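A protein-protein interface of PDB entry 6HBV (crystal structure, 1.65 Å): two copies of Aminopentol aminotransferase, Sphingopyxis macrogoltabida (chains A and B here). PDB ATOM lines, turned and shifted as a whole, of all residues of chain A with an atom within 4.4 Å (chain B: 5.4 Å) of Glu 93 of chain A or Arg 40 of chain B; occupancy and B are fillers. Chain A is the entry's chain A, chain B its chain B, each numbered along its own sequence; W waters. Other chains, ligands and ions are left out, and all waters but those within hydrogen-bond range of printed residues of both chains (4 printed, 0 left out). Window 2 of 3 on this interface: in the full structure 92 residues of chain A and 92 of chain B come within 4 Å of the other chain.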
ATOM      1  N   LEU A  84      27.078   2.990  -0.585  1.00  0.00           N
ATOM      2  CA  LEU A  84      27.194   1.547  -0.825  1.00  0.00           C
ATOM      3  C   LEU A  84      28.262   1.356  -1.907  1.00  0.00           C
ATOM      4  O   LEU A  84      29.308   0.816  -1.606  1.00  0.00           O
ATOM      5  CB  LEU A  84      25.836   0.936  -1.217  1.00  0.00           C
ATOM      6  CG  LEU A  84      24.766   1.062  -0.138  1.00  0.00           C
ATOM      7  CD1 LEU A  84      23.405   0.611  -0.661  1.00  0.00           C
ATOM      8  CD2 LEU A  84      25.145   0.275   1.118  1.00  0.00           C
ATOM      9  N   PRO A  91      27.387  -5.135 -11.554  1.00  0.00           N
ATOM     10  CA  PRO A  91      26.301  -4.239 -11.195  1.00  0.00           C
ATOM     11  C   PRO A  91      25.889  -4.445  -9.741  1.00  0.00           C
ATOM     12  O   PRO A  91      26.092  -5.496  -9.175  1.00  0.00           O
ATOM     13  CB  PRO A  91      25.147  -4.694 -12.108  1.00  0.00           C
ATOM     14  CG  PRO A  91      25.513  -6.087 -12.497  1.00  0.00           C
ATOM     15  CD  PRO A  91      27.024  -6.091 -12.603  1.00  0.00           C
ATOM     16  N   SER A  92      25.303  -3.416  -9.165  1.00  0.00           N
ATOM     17  CA  SER A  92      24.549  -3.554  -7.968  1.00  0.00           C
ATOM     18  C   SER A  92      23.305  -4.423  -8.177  1.00  0.00           C
ATOM     19  O   SER A  92      22.684  -4.430  -9.264  1.00  0.00           O
ATOM     20  CB  SER A  92      24.121  -2.239  -7.453  1.00  0.00           C
ATOM     21  OG  SER A  92      23.289  -2.414  -6.324  1.00  0.00           O
ATOM     22  N   GLU A  93      22.940  -5.154  -7.107  1.00  0.00           N
ATOM     23  CA  GLU A  93      21.627  -5.798  -7.000  1.00  0.00           C
ATOM     24  C   GLU A  93      20.492  -4.858  -7.433  1.00  0.00           C
ATOM     25  O   GLU A  93      19.464  -5.356  -7.958  1.00  0.00           O
ATOM     26  CB  GLU A  93      21.399  -6.333  -5.585  1.00  0.00           C
ATOM     27  CG  GLU A  93      21.396  -5.264  -4.511  1.00  0.00           C
ATOM     28  CD  GLU A  93      21.259  -5.797  -3.092  1.00  0.00           C
ATOM     29  OE1 GLU A  93      21.214  -7.024  -2.928  1.00  0.00           O
ATOM     30  OE2 GLU A  93      21.201  -4.975  -2.183  1.00  0.00           O
ATOM     31  N   ILE A  94      20.623  -3.536  -7.241  1.00  0.00           N
ATOM     32  CA  ILE A  94      19.492  -2.607  -7.527  1.00  0.00           C
ATOM     33  C   ILE A  94      19.230  -2.523  -9.038  1.00  0.00           C
ATOM     34  O   ILE A  94      18.186  -1.982  -9.460  1.00  0.00           O
ATOM     35  CB  ILE A  94      19.672  -1.206  -6.905  1.00  0.00           C
ATOM     36  CG1 ILE A  94      20.765  -0.387  -7.588  1.00  0.00           C
ATOM     37  CG2 ILE A  94      19.868  -1.300  -5.398  1.00  0.00           C
ATOM     38  CD1 ILE A  94      20.730   1.072  -7.269  1.00  0.00           C
ATOM     39  N   MET A  95      20.156  -3.050  -9.859  1.00  0.00           N
ATOM     40  CA  MET A  95      19.912  -3.095 -11.294  1.00  0.00           C
ATOM     41  C   MET A  95      18.658  -3.924 -11.560  1.00  0.00           C
ATOM     42  O   MET A  95      17.857  -3.597 -12.463  1.00  0.00           O
ATOM     43  CB  MET A  95      21.081  -3.690 -12.075  1.00  0.00           C
ATOM     44  CG  MET A  95      20.912  -3.669 -13.581  1.00  0.00           C
ATOM     45  SD  MET A  95      22.349  -4.415 -14.394  1.00  0.00           S
ATOM     46  CE  MET A  95      21.851  -4.171 -16.103  1.00  0.00           C
ATOM     47  N   VAL A  96      18.496  -4.991 -10.773  1.00  0.00           N
ATOM     48  CA  VAL A  96      17.342  -5.871 -10.885  1.00  0.00           C
ATOM     49  C   VAL A  96      16.101  -5.061 -10.540  1.00  0.00           C
ATOM     50  O   VAL A  96      15.122  -5.103 -11.297  1.00  0.00           O
ATOM     51  CB  VAL A  96      17.476  -7.173 -10.056  1.00  0.00           C
ATOM     52  CG1 VAL A  96      16.247  -8.059 -10.193  1.00  0.00           C
ATOM     53  CG2 VAL A  96      18.709  -7.948 -10.499  1.00  0.00           C
ATOM     54  N   ASN A  97      16.131  -4.333  -9.429  1.00  0.00           N
ATOM     55  CA  ASN A  97      14.987  -3.533  -8.994  1.00  0.00           C
ATOM     56  C   ASN A  97      14.623  -2.485 -10.042  1.00  0.00           C
ATOM     57  O   ASN A  97      13.439  -2.211 -10.287  1.00  0.00           O
ATOM     58  CB  ASN A  97      15.245  -2.833  -7.667  1.00  0.00           C
ATOM     59  CG  ASN A  97      15.393  -3.845  -6.548  1.00  0.00           C
ATOM     60  OD1 ASN A  97      16.232  -4.730  -6.620  1.00  0.00           O
ATOM     61  ND2 ASN A  97      14.579  -3.713  -5.517  1.00  0.00           N
ATOM     62  N   ARG B   6      20.852 -14.852  -1.686  1.00  0.00           N
ATOM     63  CA  ARG B   6      20.427 -13.574  -2.255  1.00  0.00           C
ATOM     64  C   ARG B   6      20.863 -13.523  -3.725  1.00  0.00           C
ATOM     65  O   ARG B   6      20.112 -13.046  -4.554  1.00  0.00           O
ATOM     66  CB  ARG B   6      20.962 -12.398  -1.444  1.00  0.00           C
ATOM     67  CG  ARG B   6      20.531 -12.449   0.018  1.00  0.00           C
ATOM     68  CD  ARG B   6      20.481 -11.088   0.667  1.00  0.00           C
ATOM     69  NE  ARG B   6      19.332 -10.325   0.193  1.00  0.00           N
ATOM     70  CZ  ARG B   6      18.957  -9.144   0.694  1.00  0.00           C
ATOM     71  NH1 ARG B   6      19.576  -8.650   1.756  1.00  0.00           N
ATOM     72  NH2 ARG B   6      17.969  -8.461   0.135  1.00  0.00           N
ATOM     73  N   LEU B  10      18.386 -13.014  -6.937  1.00  0.00           N
ATOM     74  CA  LEU B  10      18.622 -11.934  -7.865  1.00  0.00           C
ATOM     75  C   LEU B  10      18.763 -12.452  -9.295  1.00  0.00           C
ATOM     76  O   LEU B  10      18.217 -11.854 -10.192  1.00  0.00           O
ATOM     77  CB  LEU B  10      19.847 -11.133  -7.447  1.00  0.00           C
ATOM     78  CG  LEU B  10      19.623 -10.208  -6.266  1.00  0.00           C
ATOM     79  CD1 LEU B  10      20.969  -9.791  -5.698  1.00  0.00           C
ATOM     80  CD2 LEU B  10      18.796  -9.010  -6.671  1.00  0.00           C
ATOM     81  N   PHE B  38      25.935 -10.038  -8.956  1.00  0.00           N
ATOM     82  CA  PHE B  38      25.446  -8.841  -8.359  1.00  0.00           C
ATOM     83  C   PHE B  38      26.121  -8.550  -7.011  1.00  0.00           C
ATOM     84  O   PHE B  38      26.358  -9.439  -6.202  1.00  0.00           O
ATOM     85  CB  PHE B  38      23.925  -8.878  -8.209  1.00  0.00           C
ATOM     86  CG  PHE B  38      23.192  -8.969  -9.522  1.00  0.00           C
ATOM     87  CD1 PHE B  38      22.981  -7.848 -10.315  1.00  0.00           C
ATOM     88  CD2 PHE B  38      22.709 -10.192  -9.970  1.00  0.00           C
ATOM     89  CE1 PHE B  38      22.302  -7.957 -11.531  1.00  0.00           C
ATOM     90  CE2 PHE B  38      22.033 -10.301 -11.177  1.00  0.00           C
ATOM     91  CZ  PHE B  38      21.832  -9.187 -11.956  1.00  0.00           C
ATOM     92  N   PHE B  39      26.416  -7.257  -6.806  1.00  0.00           N
ATOM     93  CA  PHE B  39      27.138  -6.749  -5.635  1.00  0.00           C
ATOM     94  C   PHE B  39      26.262  -5.803  -4.815  1.00  0.00           C
ATOM     95  O   PHE B  39      25.237  -5.264  -5.305  1.00  0.00           O
ATOM     96  CB  PHE B  39      28.433  -6.099  -6.092  1.00  0.00           C
ATOM     97  CG  PHE B  39      29.341  -7.132  -6.695  1.00  0.00           C
ATOM     98  CD1 PHE B  39      29.250  -7.469  -8.029  1.00  0.00           C
ATOM     99  CD2 PHE B  39      30.279  -7.773  -5.905  1.00  0.00           C
ATOM    100  CE1 PHE B  39      30.098  -8.429  -8.562  1.00  0.00           C
ATOM    101  CE2 PHE B  39      31.117  -8.730  -6.443  1.00  0.00           C
ATOM    102  CZ  PHE B  39      31.022  -9.053  -7.770  1.00  0.00           C
ATOM    103  N   ARG B  40      26.681  -5.617  -3.561  1.00  0.00           N
ATOM    104  CA  ARG B  40      26.004  -4.693  -2.634  1.00  0.00           C
ATOM    105  C   ARG B  40      26.838  -3.424  -2.385  1.00  0.00           C
ATOM    106  O   ARG B  40      26.296  -2.300  -2.357  1.00  0.00           O
ATOM    107  CB  ARG B  40      25.664  -5.369  -1.299  1.00  0.00           C
ATOM    108  CG  ARG B  40      24.652  -4.545  -0.514  1.00  0.00           C
ATOM    109  CD  ARG B  40      23.795  -5.295   0.487  1.00  0.00           C
ATOM    110  NE  ARG B  40      22.779  -6.136  -0.123  1.00  0.00           N
ATOM    111  CZ  ARG B  40      22.642  -7.467   0.053  1.00  0.00           C
ATOM    112  NH1 ARG B  40      23.413  -8.094   0.934  1.00  0.00           N
ATOM    113  NH2 ARG B  40      21.741  -8.161  -0.644  1.00  0.00           N
ATOM    114  N   ARG B  41      28.161  -3.565  -2.189  1.00  0.00           N
ATOM    115  CA  ARG B  41      28.943  -2.391  -1.811  1.00  0.00           C
ATOM    116  C   ARG B  41      30.418  -2.553  -2.167  1.00  0.00           C
ATOM    117  O   ARG B  41      30.901  -3.648  -2.480  1.00  0.00           O
ATOM    118  CB  ARG B  41      28.736  -2.004  -0.337  1.00  0.00           C
ATOM    119  CG  ARG B  41      29.125  -3.003   0.719  1.00  0.00           C
ATOM    120  CD  ARG B  41      28.498  -2.597   2.075  1.00  0.00           C
ATOM    121  NE  ARG B  41      28.248  -3.766   2.889  1.00  0.00           N
ATOM    122  CZ  ARG B  41      29.213  -4.379   3.558  1.00  0.00           C
ATOM    123  NH1 ARG B  41      30.406  -3.800   3.625  1.00  0.00           N
ATOM    124  NH2 ARG B  41      28.996  -5.548   4.145  1.00  0.00           N
ATOM    125  N   ALA B  42      31.129  -1.414  -2.114  1.00  0.00           N
ATOM    126  CA  ALA B  42      32.505  -1.368  -2.469  1.00  0.00           C
ATOM    127  C   ALA B  42      33.228  -0.269  -1.693  1.00  0.00           C
ATOM    128  O   ALA B  42      32.697   0.811  -1.474  1.00  0.00           O
ATOM    129  CB  ALA B  42      32.661  -1.122  -3.947  1.00  0.00           C
ATOM    130  N   TRP B  48      31.829  -6.263  -1.953  1.00  0.00           N
ATOM    131  CA  TRP B  48      31.015  -7.199  -1.234  1.00  0.00           C
ATOM    132  C   TRP B  48      29.885  -7.628  -2.169  1.00  0.00           C
ATOM    133  O   TRP B  48      29.212  -6.746  -2.721  1.00  0.00           O
ATOM    134  CB  TRP B  48      30.429  -6.541   0.023  1.00  0.00           C
ATOM    135  CG  TRP B  48      31.356  -6.339   1.180  1.00  0.00           C
ATOM    136  CD1 TRP B  48      31.356  -7.091   2.323  1.00  0.00           C
ATOM    137  CD2 TRP B  48      32.395  -5.359   1.339  1.00  0.00           C
ATOM    138  NE1 TRP B  48      32.327  -6.645   3.183  1.00  0.00           N
ATOM    139  CE2 TRP B  48      32.980  -5.585   2.609  1.00  0.00           C
ATOM    140  CE3 TRP B  48      32.901  -4.315   0.553  1.00  0.00           C
ATOM    141  CZ2 TRP B  48      34.030  -4.816   3.093  1.00  0.00           C
ATOM    142  CZ3 TRP B  48      33.945  -3.549   1.034  1.00  0.00           C
ATOM    143  CH2 TRP B  48      34.502  -3.794   2.294  1.00  0.00           C
ATOM    144  N   ASP B  49      29.675  -8.939  -2.338  1.00  0.00           N
ATOM    145  CA  ASP B  49      28.572  -9.447  -3.168  1.00  0.00           C
ATOM    146  C   ASP B  49      27.235  -9.266  -2.442  1.00  0.00           C
ATOM    147  O   ASP B  49      27.154  -8.760  -1.317  1.00  0.00           O
ATOM    148  CB  ASP B  49      28.822 -10.877  -3.650  1.00  0.00           C
ATOM    149  CG  ASP B  49      28.905 -11.906  -2.535  1.00  0.00           C
ATOM    150  OD1 ASP B  49      28.450 -11.564  -1.416  1.00  0.00           O
ATOM    151  OD2 ASP B  49      29.422 -13.021  -2.818  1.00  0.00           O
ATOM    152  N   ALA B  50      26.153  -9.686  -3.107  1.00  0.00           N
ATOM    153  CA  ALA B  50      24.824  -9.515  -2.566  1.00  0.00           C
ATOM    154  C   ALA B  50      24.635 -10.316  -1.260  1.00  0.00           C
ATOM    155  O   ALA B  50      23.753 -10.010  -0.485  1.00  0.00           O
ATOM    156  CB  ALA B  50      23.813  -9.913  -3.621  1.00  0.00           C
ATOM    157  N   ASP B  51      25.456 -11.338  -1.006  1.00  0.00           N
ATOM    158  CA  ASP B  51      25.388 -12.136   0.246  1.00  0.00           C
ATOM    159  C   ASP B  51      26.441 -11.640   1.270  1.00  0.00           C
ATOM    160  O   ASP B  51      26.788 -12.348   2.186  1.00  0.00           O
ATOM    161  CB  ASP B  51      25.535 -13.607  -0.112  1.00  0.00           C
ATOM    162  CG  ASP B  51      24.302 -14.145  -0.829  1.00  0.00           C
ATOM    163  OD1 ASP B  51      23.290 -14.381  -0.141  1.00  0.00           O
ATOM    164  OD2 ASP B  51      24.355 -14.317  -2.059  1.00  0.00           O
ATOM    165  N   GLU B  52      26.936 -10.417   1.090  1.00  0.00           N
ATOM    166  CA  GLU B  52      27.857  -9.672   2.008  1.00  0.00           C
ATOM    167  C   GLU B  52      29.216 -10.385   2.184  1.00  0.00           C
ATOM    168  O   GLU B  52      29.889 -10.174   3.186  1.00  0.00           O
ATOM    169  CB  GLU B  52      27.204  -9.429   3.373  1.00  0.00           C
ATOM    170  CG  GLU B  52      25.865  -8.722   3.311  1.00  0.00           C
ATOM    171  CD  GLU B  52      25.910  -7.225   3.082  1.00  0.00           C
ATOM    172  OE1 GLU B  52      27.004  -6.656   2.897  1.00  0.00           O
ATOM    173  OE2 GLU B  52      24.848  -6.623   3.090  1.00  0.00           O
HETATM  174  O   HOH W   1      19.411  -5.348  -0.292  1.00  0.00           O
HETATM  175  O   HOH W   2      18.923  -8.593  -2.748  1.00  0.00           O
HETATM  176  O   HOH W   3      24.110  -1.737  -3.770  1.00  0.00           O
HETATM  177  O   HOH W   4      30.867   1.220   0.764  1.00  0.00           O
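NH2 of Arg 41 of chain B lies within salt-bridge range of OE1 of Glu 52 of chain B.
The guanidinium group of Arg 40 of chain B lies within salt-bridge range of the side-chain carboxylate of Glu 52 of chain B.
The backbone carbonyl oxygen (O) of Arg 41 of chain B lies within hydrogen-bond range of the backbone NH (N) of Trp 48 of chain B, 2.8 Å away.
NH1 of Arg 40 of chain B sits at hydrogen-bond distance from O of Ala 50 of chain B (2.4 Å).
N of Ile 94 of chain A sits close to OG of Ser 92 of chain A (3.0 Å).
O of Phe 38 of chain B is in hydrogen-bond range of N of Ala 50 of chain B.
No position is printed for both chains.
Of the 13 pairs that touch across the chains among the printed residues, none has its exchanged pair printed and touching as well.
Water W1 lies within hydrogen-bond range of OE2 of Glu 93 of chain A (2.6 Å), NH2 of Arg 6 of chain B (3.5 Å) and NE of Arg 40 of chain B (3.5 Å).
Water W3 bridges the backbone carbonyl oxygen (O) of Arg 40 of chain B and the side-chain hydroxyl (OG) of Ser 92 of chain A.
Water W2 bridges OE1 of Glu 93 of chain A (2.8 Å) and NH2 of Arg 6 of chain B (3.0 Å).
Water W4 bridges the backbone carbonyl oxygen of Leu 84 of chain A (2.9 Å) and the backbone carbonyl oxygen of Ala 42 of chain B (2.9 Å).
Of the 8 printed residues of chain A, 5 touch a printed residue of chain B.
Printed residues of chain A within 4 Å of Phe 39 of chain B: Pro 91 (3.0 Å), Ser 92 (3.2 Å) and Glu 93 (2.9 Å).
Of chain A, only Leu 84 (3.5 Å) and Glu 93 (2.6 Å) come within 4 Å of Arg 40 of chain B.
Of the printed residues of chain A, Ala 50 of chain B touches Glu 93 (3.9 Å).
Asp 51 of chain B touches none of the printed residues of chain A.
The nearest printed residue of chain B that does not touch Glu 93 of chain A is Phe 38 of chain B (4.01 Å).
The nearest printed residue of chain A that does not touch Arg 40 of chain B is Ser 92 of chain A (5.0 Å).
Among the printed residues, pairs that only touch across the chains: Leu 84 of chain A with Arg 40 of chain B (3.5 Å), Leu 84 of chain A with Arg 41 of chain B (3.1 Å), Pro 91 of chain A with Phe 38 of chain B (3.5 Å), Ser 92 of chain A with Phe 38 of chain B (3.6 Å), Ser 92 of chain A with Phe 39 of chain B (3.2 Å), Glu 93 of chain A with Leu 10 of chain B (3.5 Å), Glu 93 of chain A with Ala 50 of chain B (3.9 Å), Val 96 of chain A with Leu 10 of chain B (3.9 Å) and Val 96 of chain A with Phe 38 of chain B (3.7 Å).
O of Leu 84 of chain A lies within hydrogen-bond range of N of Ala 42 of chain B.
The backbone NH of Phe 39 of chain B sits at hydrogen-bond distance from the backbone carbonyl oxygen of Pro 91 of chain A, at 3.0 Å.
OE1 of Glu 93 of chain A is in salt-bridge range of NH2 of Arg 40 of chain B, at 2.6 Å.
N of Glu 93 of chain A is in hydrogen-bond range of O of Phe 39 of chain B (2.9 Å).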
